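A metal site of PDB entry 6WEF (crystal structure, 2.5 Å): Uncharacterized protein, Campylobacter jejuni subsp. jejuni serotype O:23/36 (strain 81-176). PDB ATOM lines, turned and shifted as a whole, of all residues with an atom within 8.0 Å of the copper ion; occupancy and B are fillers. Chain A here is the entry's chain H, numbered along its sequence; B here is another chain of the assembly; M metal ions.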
ATOM      1  N   VAL A  20      15.333 -13.728  14.314  1.00  0.00           N
ATOM      2  CA  VAL A  20      15.737 -15.133  14.240  1.00  0.00           C
ATOM      3  C   VAL A  20      16.057 -15.450  12.784  1.00  0.00           C
ATOM      4  O   VAL A  20      15.708 -14.705  11.869  1.00  0.00           O
ATOM      5  CB  VAL A  20      14.638 -16.083  14.777  1.00  0.00           C
ATOM      6  CG1 VAL A  20      14.167 -15.646  16.159  1.00  0.00           C
ATOM      7  CG2 VAL A  20      13.460 -16.157  13.813  1.00  0.00           C
ATOM      8  N   LEU A  22      16.648 -19.159  10.121  1.00  0.00           N
ATOM      9  CA  LEU A  22      16.567 -20.605  10.012  1.00  0.00           C
ATOM     10  C   LEU A  22      17.274 -21.107   8.760  1.00  0.00           C
ATOM     11  O   LEU A  22      17.976 -20.347   8.094  1.00  0.00           O
ATOM     12  CB  LEU A  22      15.100 -21.055   9.968  1.00  0.00           C
ATOM     13  CG  LEU A  22      14.132 -20.613  11.077  1.00  0.00           C
ATOM     14  CD1 LEU A  22      13.781 -19.139  10.974  1.00  0.00           C
ATOM     15  CD2 LEU A  22      12.877 -21.474  11.017  1.00  0.00           C
ATOM     16  N   GLN A  23      17.073 -22.387   8.439  1.00  0.00           N
ATOM     17  CA  GLN A  23      17.496 -22.907   7.155  1.00  0.00           C
ATOM     18  C   GLN A  23      16.690 -22.237   6.042  1.00  0.00           C
ATOM     19  O   GLN A  23      15.622 -21.684   6.287  1.00  0.00           O
ATOM     20  CB  GLN A  23      17.289 -24.425   7.094  1.00  0.00           C
ATOM     21  CG  GLN A  23      18.185 -25.223   8.024  1.00  0.00           C
ATOM     22  CD  GLN A  23      18.193 -26.705   7.687  1.00  0.00           C
ATOM     23  OE1 GLN A  23      19.017 -27.172   6.896  1.00  0.00           O
ATOM     24  NE2 GLN A  23      17.270 -27.448   8.281  1.00  0.00           N
ATOM     25  N   ILE A  25      13.967 -21.748   3.426  1.00  0.00           N
ATOM     26  CA  ILE A  25      12.597 -22.226   3.528  1.00  0.00           C
ATOM     27  C   ILE A  25      11.944 -22.226   2.158  1.00  0.00           C
ATOM     28  O   ILE A  25      12.123 -21.280   1.377  1.00  0.00           O
ATOM     29  CB  ILE A  25      11.784 -21.353   4.506  1.00  0.00           C
ATOM     30  CG1 ILE A  25      12.348 -21.447   5.928  1.00  0.00           C
ATOM     31  CG2 ILE A  25      10.325 -21.762   4.481  1.00  0.00           C
ATOM     32  CD1 ILE A  25      12.474 -22.869   6.463  1.00  0.00           C
ATOM     33  N   GLU A  26      11.197 -23.277   1.864  1.00  0.00           N
ATOM     34  CA  GLU A  26      10.398 -23.337   0.653  1.00  0.00           C
ATOM     35  C   GLU A  26       9.133 -22.508   0.839  1.00  0.00           C
ATOM     36  O   GLU A  26       8.404 -22.686   1.819  1.00  0.00           O
ATOM     37  CB  GLU A  26      10.051 -24.783   0.315  1.00  0.00           C
ATOM     38  CG  GLU A  26       9.613 -24.998  -1.120  1.00  0.00           C
ATOM     39  CD  GLU A  26       9.398 -26.457  -1.452  1.00  0.00           C
ATOM     40  OE1 GLU A  26      10.026 -27.314  -0.806  1.00  0.00           O
ATOM     41  OE2 GLU A  26       8.580 -26.740  -2.360  1.00  0.00           O
ATOM     42  N   MET A  27       8.868 -21.611  -0.110  1.00  0.00           N
ATOM     43  CA  MET A  27       7.824 -20.612   0.029  1.00  0.00           C
ATOM     44  C   MET A  27       6.824 -20.698  -1.113  1.00  0.00           C
ATOM     45  O   MET A  27       7.171 -21.042  -2.244  1.00  0.00           O
ATOM     46  CB  MET A  27       8.431 -19.198   0.071  1.00  0.00           C
ATOM     47  CG  MET A  27       9.008 -18.814   1.413  1.00  0.00           C
ATOM     48  SD  MET A  27       7.749 -18.243   2.568  1.00  0.00           S
ATOM     49  CE  MET A  27       7.264 -16.694   1.801  1.00  0.00           C
ATOM     50  N   ASP A  33       9.724 -14.678  -3.335  1.00  0.00           N
ATOM     51  CA  ASP A  33      10.985 -14.644  -2.622  1.00  0.00           C
ATOM     52  C   ASP A  33      12.028 -15.503  -3.319  1.00  0.00           C
ATOM     53  O   ASP A  33      11.704 -16.375  -4.132  1.00  0.00           O
ATOM     54  CB  ASP A  33      10.800 -15.109  -1.181  1.00  0.00           C
ATOM     55  CG  ASP A  33      11.965 -14.727  -0.282  1.00  0.00           C
ATOM     56  OD1 ASP A  33      12.725 -13.797  -0.645  1.00  0.00           O
ATOM     57  OD2 ASP A  33      12.127 -15.363   0.775  1.00  0.00           O
ATOM     58  N   HIS A  42      17.294 -18.253   6.178  1.00  0.00           N
ATOM     59  CA  HIS A  42      15.952 -17.693   6.071  1.00  0.00           C
ATOM     60  C   HIS A  42      15.805 -16.700   7.227  1.00  0.00           C
ATOM     61  O   HIS A  42      15.436 -17.090   8.336  1.00  0.00           O
ATOM     62  CB  HIS A  42      14.886 -18.767   6.104  1.00  0.00           C
ATOM     63  CG  HIS A  42      13.493 -18.248   5.877  1.00  0.00           C
ATOM     64  ND1 HIS A  42      13.068 -17.776   4.651  1.00  0.00           N
ATOM     65  CD2 HIS A  42      12.447 -18.120   6.722  1.00  0.00           C
ATOM     66  CE1 HIS A  42      11.810 -17.386   4.765  1.00  0.00           C
ATOM     67  NE2 HIS A  42      11.413 -17.586   6.004  1.00  0.00           N
ATOM     68  N   LEU A  43      16.102 -15.438   6.959  1.00  0.00           N
ATOM     69  CA  LEU A  43      16.023 -14.398   7.982  1.00  0.00           C
ATOM     70  C   LEU A  43      14.575 -14.094   8.317  1.00  0.00           C
ATOM     71  O   LEU A  43      13.713 -14.024   7.436  1.00  0.00           O
ATOM     72  CB  LEU A  43      16.740 -13.134   7.512  1.00  0.00           C
ATOM     73  CG  LEU A  43      16.686 -11.917   8.433  1.00  0.00           C
ATOM     74  CD1 LEU A  43      17.487 -12.156   9.705  1.00  0.00           C
ATOM     75  CD2 LEU A  43      17.206 -10.680   7.690  1.00  0.00           C
ATOM     76  N   GLU A  44      14.293 -13.905   9.602  1.00  0.00           N
ATOM     77  CA  GLU A  44      12.937 -13.639  10.073  1.00  0.00           C
ATOM     78  C   GLU A  44      12.961 -12.505  11.086  1.00  0.00           C
ATOM     79  O   GLU A  44      13.979 -12.230  11.734  1.00  0.00           O
ATOM     80  CB  GLU A  44      12.311 -14.892  10.694  1.00  0.00           C
ATOM     81  CG  GLU A  44      11.615 -15.802   9.695  1.00  0.00           C
ATOM     82  CD  GLU A  44      11.031 -17.045  10.330  1.00  0.00           C
ATOM     83  OE1 GLU A  44      11.251 -18.149   9.788  1.00  0.00           O
ATOM     84  OE2 GLU A  44      10.341 -16.918  11.365  1.00  0.00           O
ATOM     85  N   ALA A  45      11.813 -11.842  11.224  1.00  0.00           N
ATOM     86  CA  ALA A  45      11.623 -10.781  12.204  1.00  0.00           C
ATOM     87  C   ALA A  45      10.276 -10.995  12.879  1.00  0.00           C
ATOM     88  O   ALA A  45       9.247 -11.034  12.210  1.00  0.00           O
ATOM     89  CB  ALA A  45      11.684  -9.400  11.557  1.00  0.00           C
ATOM     90  N   MET A  86       9.296 -10.056   3.720  1.00  0.00           N
ATOM     91  CA  MET A  86       7.943 -10.182   3.210  1.00  0.00           C
ATOM     92  C   MET A  86       7.028 -10.833   4.250  1.00  0.00           C
ATOM     93  O   MET A  86       7.486 -11.674   5.035  1.00  0.00           O
ATOM     94  CB  MET A  86       7.914 -11.025   1.932  1.00  0.00           C
ATOM     95  CG  MET A  86       8.722 -10.429   0.788  1.00  0.00           C
ATOM     96  SD  MET A  86      10.418 -11.059   0.736  1.00  0.00           S
ATOM     97  CE  MET A  86      10.906 -10.601  -0.929  1.00  0.00           C
ATOM     98  N   PRO A  87       5.752 -10.476   4.280  1.00  0.00           N
ATOM     99  CA  PRO A  87       4.830 -11.101   5.240  1.00  0.00           C
ATOM    100  C   PRO A  87       4.517 -12.535   4.836  1.00  0.00           C
ATOM    101  O   PRO A  87       4.304 -12.831   3.660  1.00  0.00           O
ATOM    102  CB  PRO A  87       3.587 -10.213   5.183  1.00  0.00           C
ATOM    103  CG  PRO A  87       3.606  -9.636   3.800  1.00  0.00           C
ATOM    104  CD  PRO A  87       5.069  -9.470   3.442  1.00  0.00           C
ATOM    105  N   MET A  88       4.488 -13.423   5.823  1.00  0.00           N
ATOM    106  CA  MET A  88       4.201 -14.827   5.582  1.00  0.00           C
ATOM    107  C   MET A  88       3.777 -15.464   6.901  1.00  0.00           C
ATOM    108  O   MET A  88       3.714 -14.804   7.944  1.00  0.00           O
ATOM    109  CB  MET A  88       5.418 -15.542   4.990  1.00  0.00           C
ATOM    110  CG  MET A  88       6.594 -15.664   5.944  1.00  0.00           C
ATOM    111  SD  MET A  88       8.117 -16.150   5.120  1.00  0.00           S
ATOM    112  CE  MET A  88       8.447 -14.689   4.123  1.00  0.00           C
ATOM    113  N   VAL A  89       3.489 -16.763   6.836  1.00  0.00           N
ATOM    114  CA  VAL A  89       3.024 -17.514   7.996  1.00  0.00           C
ATOM    115  C   VAL A  89       3.632 -18.906   7.952  1.00  0.00           C
ATOM    116  O   VAL A  89       3.748 -19.521   6.897  1.00  0.00           O
ATOM    117  CB  VAL A  89       1.479 -17.600   8.045  1.00  0.00           C
ATOM    118  CG1 VAL A  89       0.948 -18.349   6.836  1.00  0.00           C
ATOM    119  CG2 VAL A  89       1.023 -18.251   9.340  1.00  0.00           C
ATOM    120  N   ALA A  90       4.022 -19.406   9.128  1.00  0.00           N
ATOM    121  CA  ALA A  90       4.540 -20.758   9.269  1.00  0.00           C
ATOM    122  C   ALA A  90       3.747 -21.485  10.355  1.00  0.00           C
ATOM    123  O   ALA A  90       2.733 -20.969  10.822  1.00  0.00           O
ATOM    124  CB  ALA A  90       6.031 -20.747   9.603  1.00  0.00           C
ATOM    125  N   GLY A  93       2.894 -19.260  13.382  1.00  0.00           N
ATOM    126  CA  GLY A  93       2.160 -18.020  13.256  1.00  0.00           C
ATOM    127  C   GLY A  93       2.771 -17.087  12.229  1.00  0.00           C
ATOM    128  O   GLY A  93       3.838 -17.354  11.673  1.00  0.00           O
ATOM    129  N   PRO A  94       2.116 -15.964  11.976  1.00  0.00           N
ATOM    130  CA  PRO A  94       2.608 -15.031  10.961  1.00  0.00           C
ATOM    131  C   PRO A  94       3.899 -14.361  11.381  1.00  0.00           C
ATOM    132  O   PRO A  94       4.273 -14.325  12.565  1.00  0.00           O
ATOM    133  CB  PRO A  94       1.468 -14.006  10.833  1.00  0.00           C
ATOM    134  CG  PRO A  94       0.778 -14.048  12.165  1.00  0.00           C
ATOM    135  CD  PRO A  94       0.873 -15.486  12.616  1.00  0.00           C
ATOM    136  N   HIS A  95       4.597 -13.822  10.386  1.00  0.00           N
ATOM    137  CA  HIS A  95       5.871 -13.137  10.619  1.00  0.00           C
ATOM    138  C   HIS A  95       6.360 -12.517   9.318  1.00  0.00           C
ATOM    139  O   HIS A  95       5.714 -12.641   8.281  1.00  0.00           O
ATOM    140  CB  HIS A  95       6.909 -14.120  11.164  1.00  0.00           C
ATOM    141  CG  HIS A  95       7.277 -15.204  10.197  1.00  0.00           C
ATOM    142  ND1 HIS A  95       6.642 -16.426  10.181  1.00  0.00           N
ATOM    143  CD2 HIS A  95       8.211 -15.236   9.222  1.00  0.00           C
ATOM    144  CE1 HIS A  95       7.172 -17.169   9.226  1.00  0.00           C
ATOM    145  NE2 HIS A  95       8.122 -16.484   8.633  1.00  0.00           N
ATOM    146  N   TYR A  96       7.510 -11.858   9.376  1.00  0.00           N
ATOM    147  CA  TYR A  96       8.177 -11.330   8.194  1.00  0.00           C
ATOM    148  C   TYR A  96       9.476 -12.083   7.983  1.00  0.00           C
ATOM    149  O   TYR A  96      10.267 -12.233   8.927  1.00  0.00           O
ATOM    150  CB  TYR A  96       8.449  -9.829   8.332  1.00  0.00           C
ATOM    151  CG  TYR A  96       7.210  -8.990   8.579  1.00  0.00           C
ATOM    152  CD1 TYR A  96       6.528  -8.403   7.510  1.00  0.00           C
ATOM    153  CD2 TYR A  96       6.729  -8.787   9.858  1.00  0.00           C
ATOM    154  CE1 TYR A  96       5.401  -7.627   7.727  1.00  0.00           C
ATOM    155  CE2 TYR A  96       5.603  -8.015  10.088  1.00  0.00           C
ATOM    156  CZ  TYR A  96       4.948  -7.442   9.020  1.00  0.00           C
ATOM    157  OH  TYR A  96       3.825  -6.679   9.247  1.00  0.00           O
ATOM    158  N   GLY A  97       9.698 -12.562   6.768  1.00  0.00           N
ATOM    159  CA  GLY A  97      10.863 -13.380   6.482  1.00  0.00           C
ATOM    160  C   GLY A  97      11.365 -13.173   5.071  1.00  0.00           C
ATOM    161  O   GLY A  97      10.772 -12.439   4.272  1.00  0.00           O
ATOM    162  N   ALA A  98      12.478 -13.834   4.766  1.00  0.00           N
ATOM    163  CA  ALA A  98      13.099 -13.742   3.449  1.00  0.00           C
ATOM    164  C   ALA A  98      14.226 -14.744   3.369  1.00  0.00           C
ATOM    165  O   ALA A  98      14.940 -14.956   4.352  1.00  0.00           O
ATOM    166  CB  ALA A  98      13.627 -12.323   3.180  1.00  0.00           C
ATOM    167  N   ASN A  99      14.372 -15.379   2.208  1.00  0.00           N
ATOM    168  CA  ASN A  99      15.521 -16.214   1.926  1.00  0.00           C
ATOM    169  C   ASN A  99      16.659 -15.340   1.420  1.00  0.00           C
ATOM    170  O   ASN A  99      16.465 -14.522   0.513  1.00  0.00           O
ATOM    171  CB  ASN A  99      15.182 -17.278   0.882  1.00  0.00           C
ATOM    172  CG  ASN A  99      14.372 -18.423   1.465  1.00  0.00           C
ATOM    173  OD1 ASN A  99      14.475 -18.736   2.652  1.00  0.00           O
ATOM    174  ND2 ASN A  99      13.558 -19.054   0.632  1.00  0.00           N
ATOM    175  N   GLY B 130       2.899 -14.890   1.915  1.00  0.00           N
ATOM    176  CA  GLY B 130       3.516 -16.189   1.713  1.00  0.00           C
ATOM    177  C   GLY B 130       3.229 -17.160   2.846  1.00  0.00           C
ATOM    178  O   GLY B 130       2.659 -16.814   3.880  1.00  0.00           O
ATOM    179  N   ARG B 131       3.648 -18.402   2.637  1.00  0.00           N
ATOM    180  CA  ARG B 131       3.499 -19.447   3.637  1.00  0.00           C
ATOM    181  C   ARG B 131       4.613 -20.473   3.454  1.00  0.00           C
ATOM    182  O   ARG B 131       4.921 -20.879   2.336  1.00  0.00           O
ATOM    183  CB  ARG B 131       2.139 -20.125   3.555  1.00  0.00           C
ATOM    184  CG  ARG B 131       1.787 -20.665   2.180  1.00  0.00           C
ATOM    185  CD  ARG B 131       0.658 -21.707   2.252  1.00  0.00           C
ATOM    186  NE  ARG B 131       0.381 -22.274   0.928  1.00  0.00           N
ATOM    187  CZ  ARG B 131       0.388 -23.575   0.648  1.00  0.00           C
ATOM    188  NH1 ARG B 131       0.655 -24.478   1.581  1.00  0.00           N
ATOM    189  NH2 ARG B 131       0.125 -23.966  -0.591  1.00  0.00           N
ATOM    190  N   HIS B 132       5.225 -20.875   4.565  1.00  0.00           N
ATOM    191  CA  HIS B 132       6.180 -21.966   4.540  1.00  0.00           C
ATOM    192  C   HIS B 132       5.484 -23.231   4.046  1.00  0.00           C
ATOM    193  O   HIS B 132       4.393 -23.578   4.521  1.00  0.00           O
ATOM    194  CB  HIS B 132       6.770 -22.204   5.922  1.00  0.00           C
ATOM    195  CG  HIS B 132       7.553 -21.045   6.455  1.00  0.00           C
ATOM    196  ND1 HIS B 132       8.536 -21.190   7.413  1.00  0.00           N
ATOM    197  CD2 HIS B 132       7.507 -19.717   6.174  1.00  0.00           C
ATOM    198  CE1 HIS B 132       9.061 -20.009   7.695  1.00  0.00           C
ATOM    199  NE2 HIS B 132       8.448 -19.104   6.959  1.00  0.00           N
ATOM    200  N   THR B 137       8.447 -26.761   9.012  1.00  0.00           N
ATOM    201  CA  THR B 137       7.780 -25.542   9.460  1.00  0.00           C
ATOM    202  C   THR B 137       6.619 -25.137   8.572  1.00  0.00           C
ATOM    203  O   THR B 137       6.089 -24.026   8.728  1.00  0.00           O
ATOM    204  CB  THR B 137       8.785 -24.382   9.535  1.00  0.00           C
ATOM    205  OG1 THR B 137       9.167 -23.999   8.205  1.00  0.00           O
ATOM    206  CG2 THR B 137      10.029 -24.789  10.318  1.00  0.00           C
HETATM  207 CU    CU M   1       9.668 -17.186   7.112  1.00  0.00          CU
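The copper ion is bound by NE2 of His 42, at 2.1 Å.
NE2 of His 132 of chain B binds the copper ion (2.3 Å).
NE2 of His 95 binds the copper ion, 2.3 Å away.
SD of Met 88 is bound to the copper ion (2.7 Å).
Glu 44 touches the copper ion.
Within 4 Å of the copper ion: His 42, Glu 44, Met 88, His 95 and His 132 of chain B.
The nearest printed residue that does not touch the copper ion is Gly 97 (4.04 Å).
A ring nitrogen (ND1) of His 42 lies close to the backbone carbonyl oxygen (O) of Ala 98.
The backbone NH (N) of His 42 sits at hydrogen-bond distance from the backbone carbonyl oxygen (O) of Leu 22.
A ring nitrogen (ND1) of His 42 lies within hydrogen-bond range of the side-chain amide oxygen (OD1) of Asn 99 (2.6 Å).
N of His 132 of chain B lies within hydrogen-bond range of O of Val 89, 3.1 Å away.
OG1 of Thr 137 of chain B is in hydrogen-bond range of ND1 of His 132 of chain B, at 3.0 Å.
ND1 of His 95 is in hydrogen-bond range of O of Gly 93 (3.3 Å).
The backbone NH of Glu 44 is in hydrogen-bond range of the backbone carbonyl oxygen of Val 20, at 2.8 Å.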
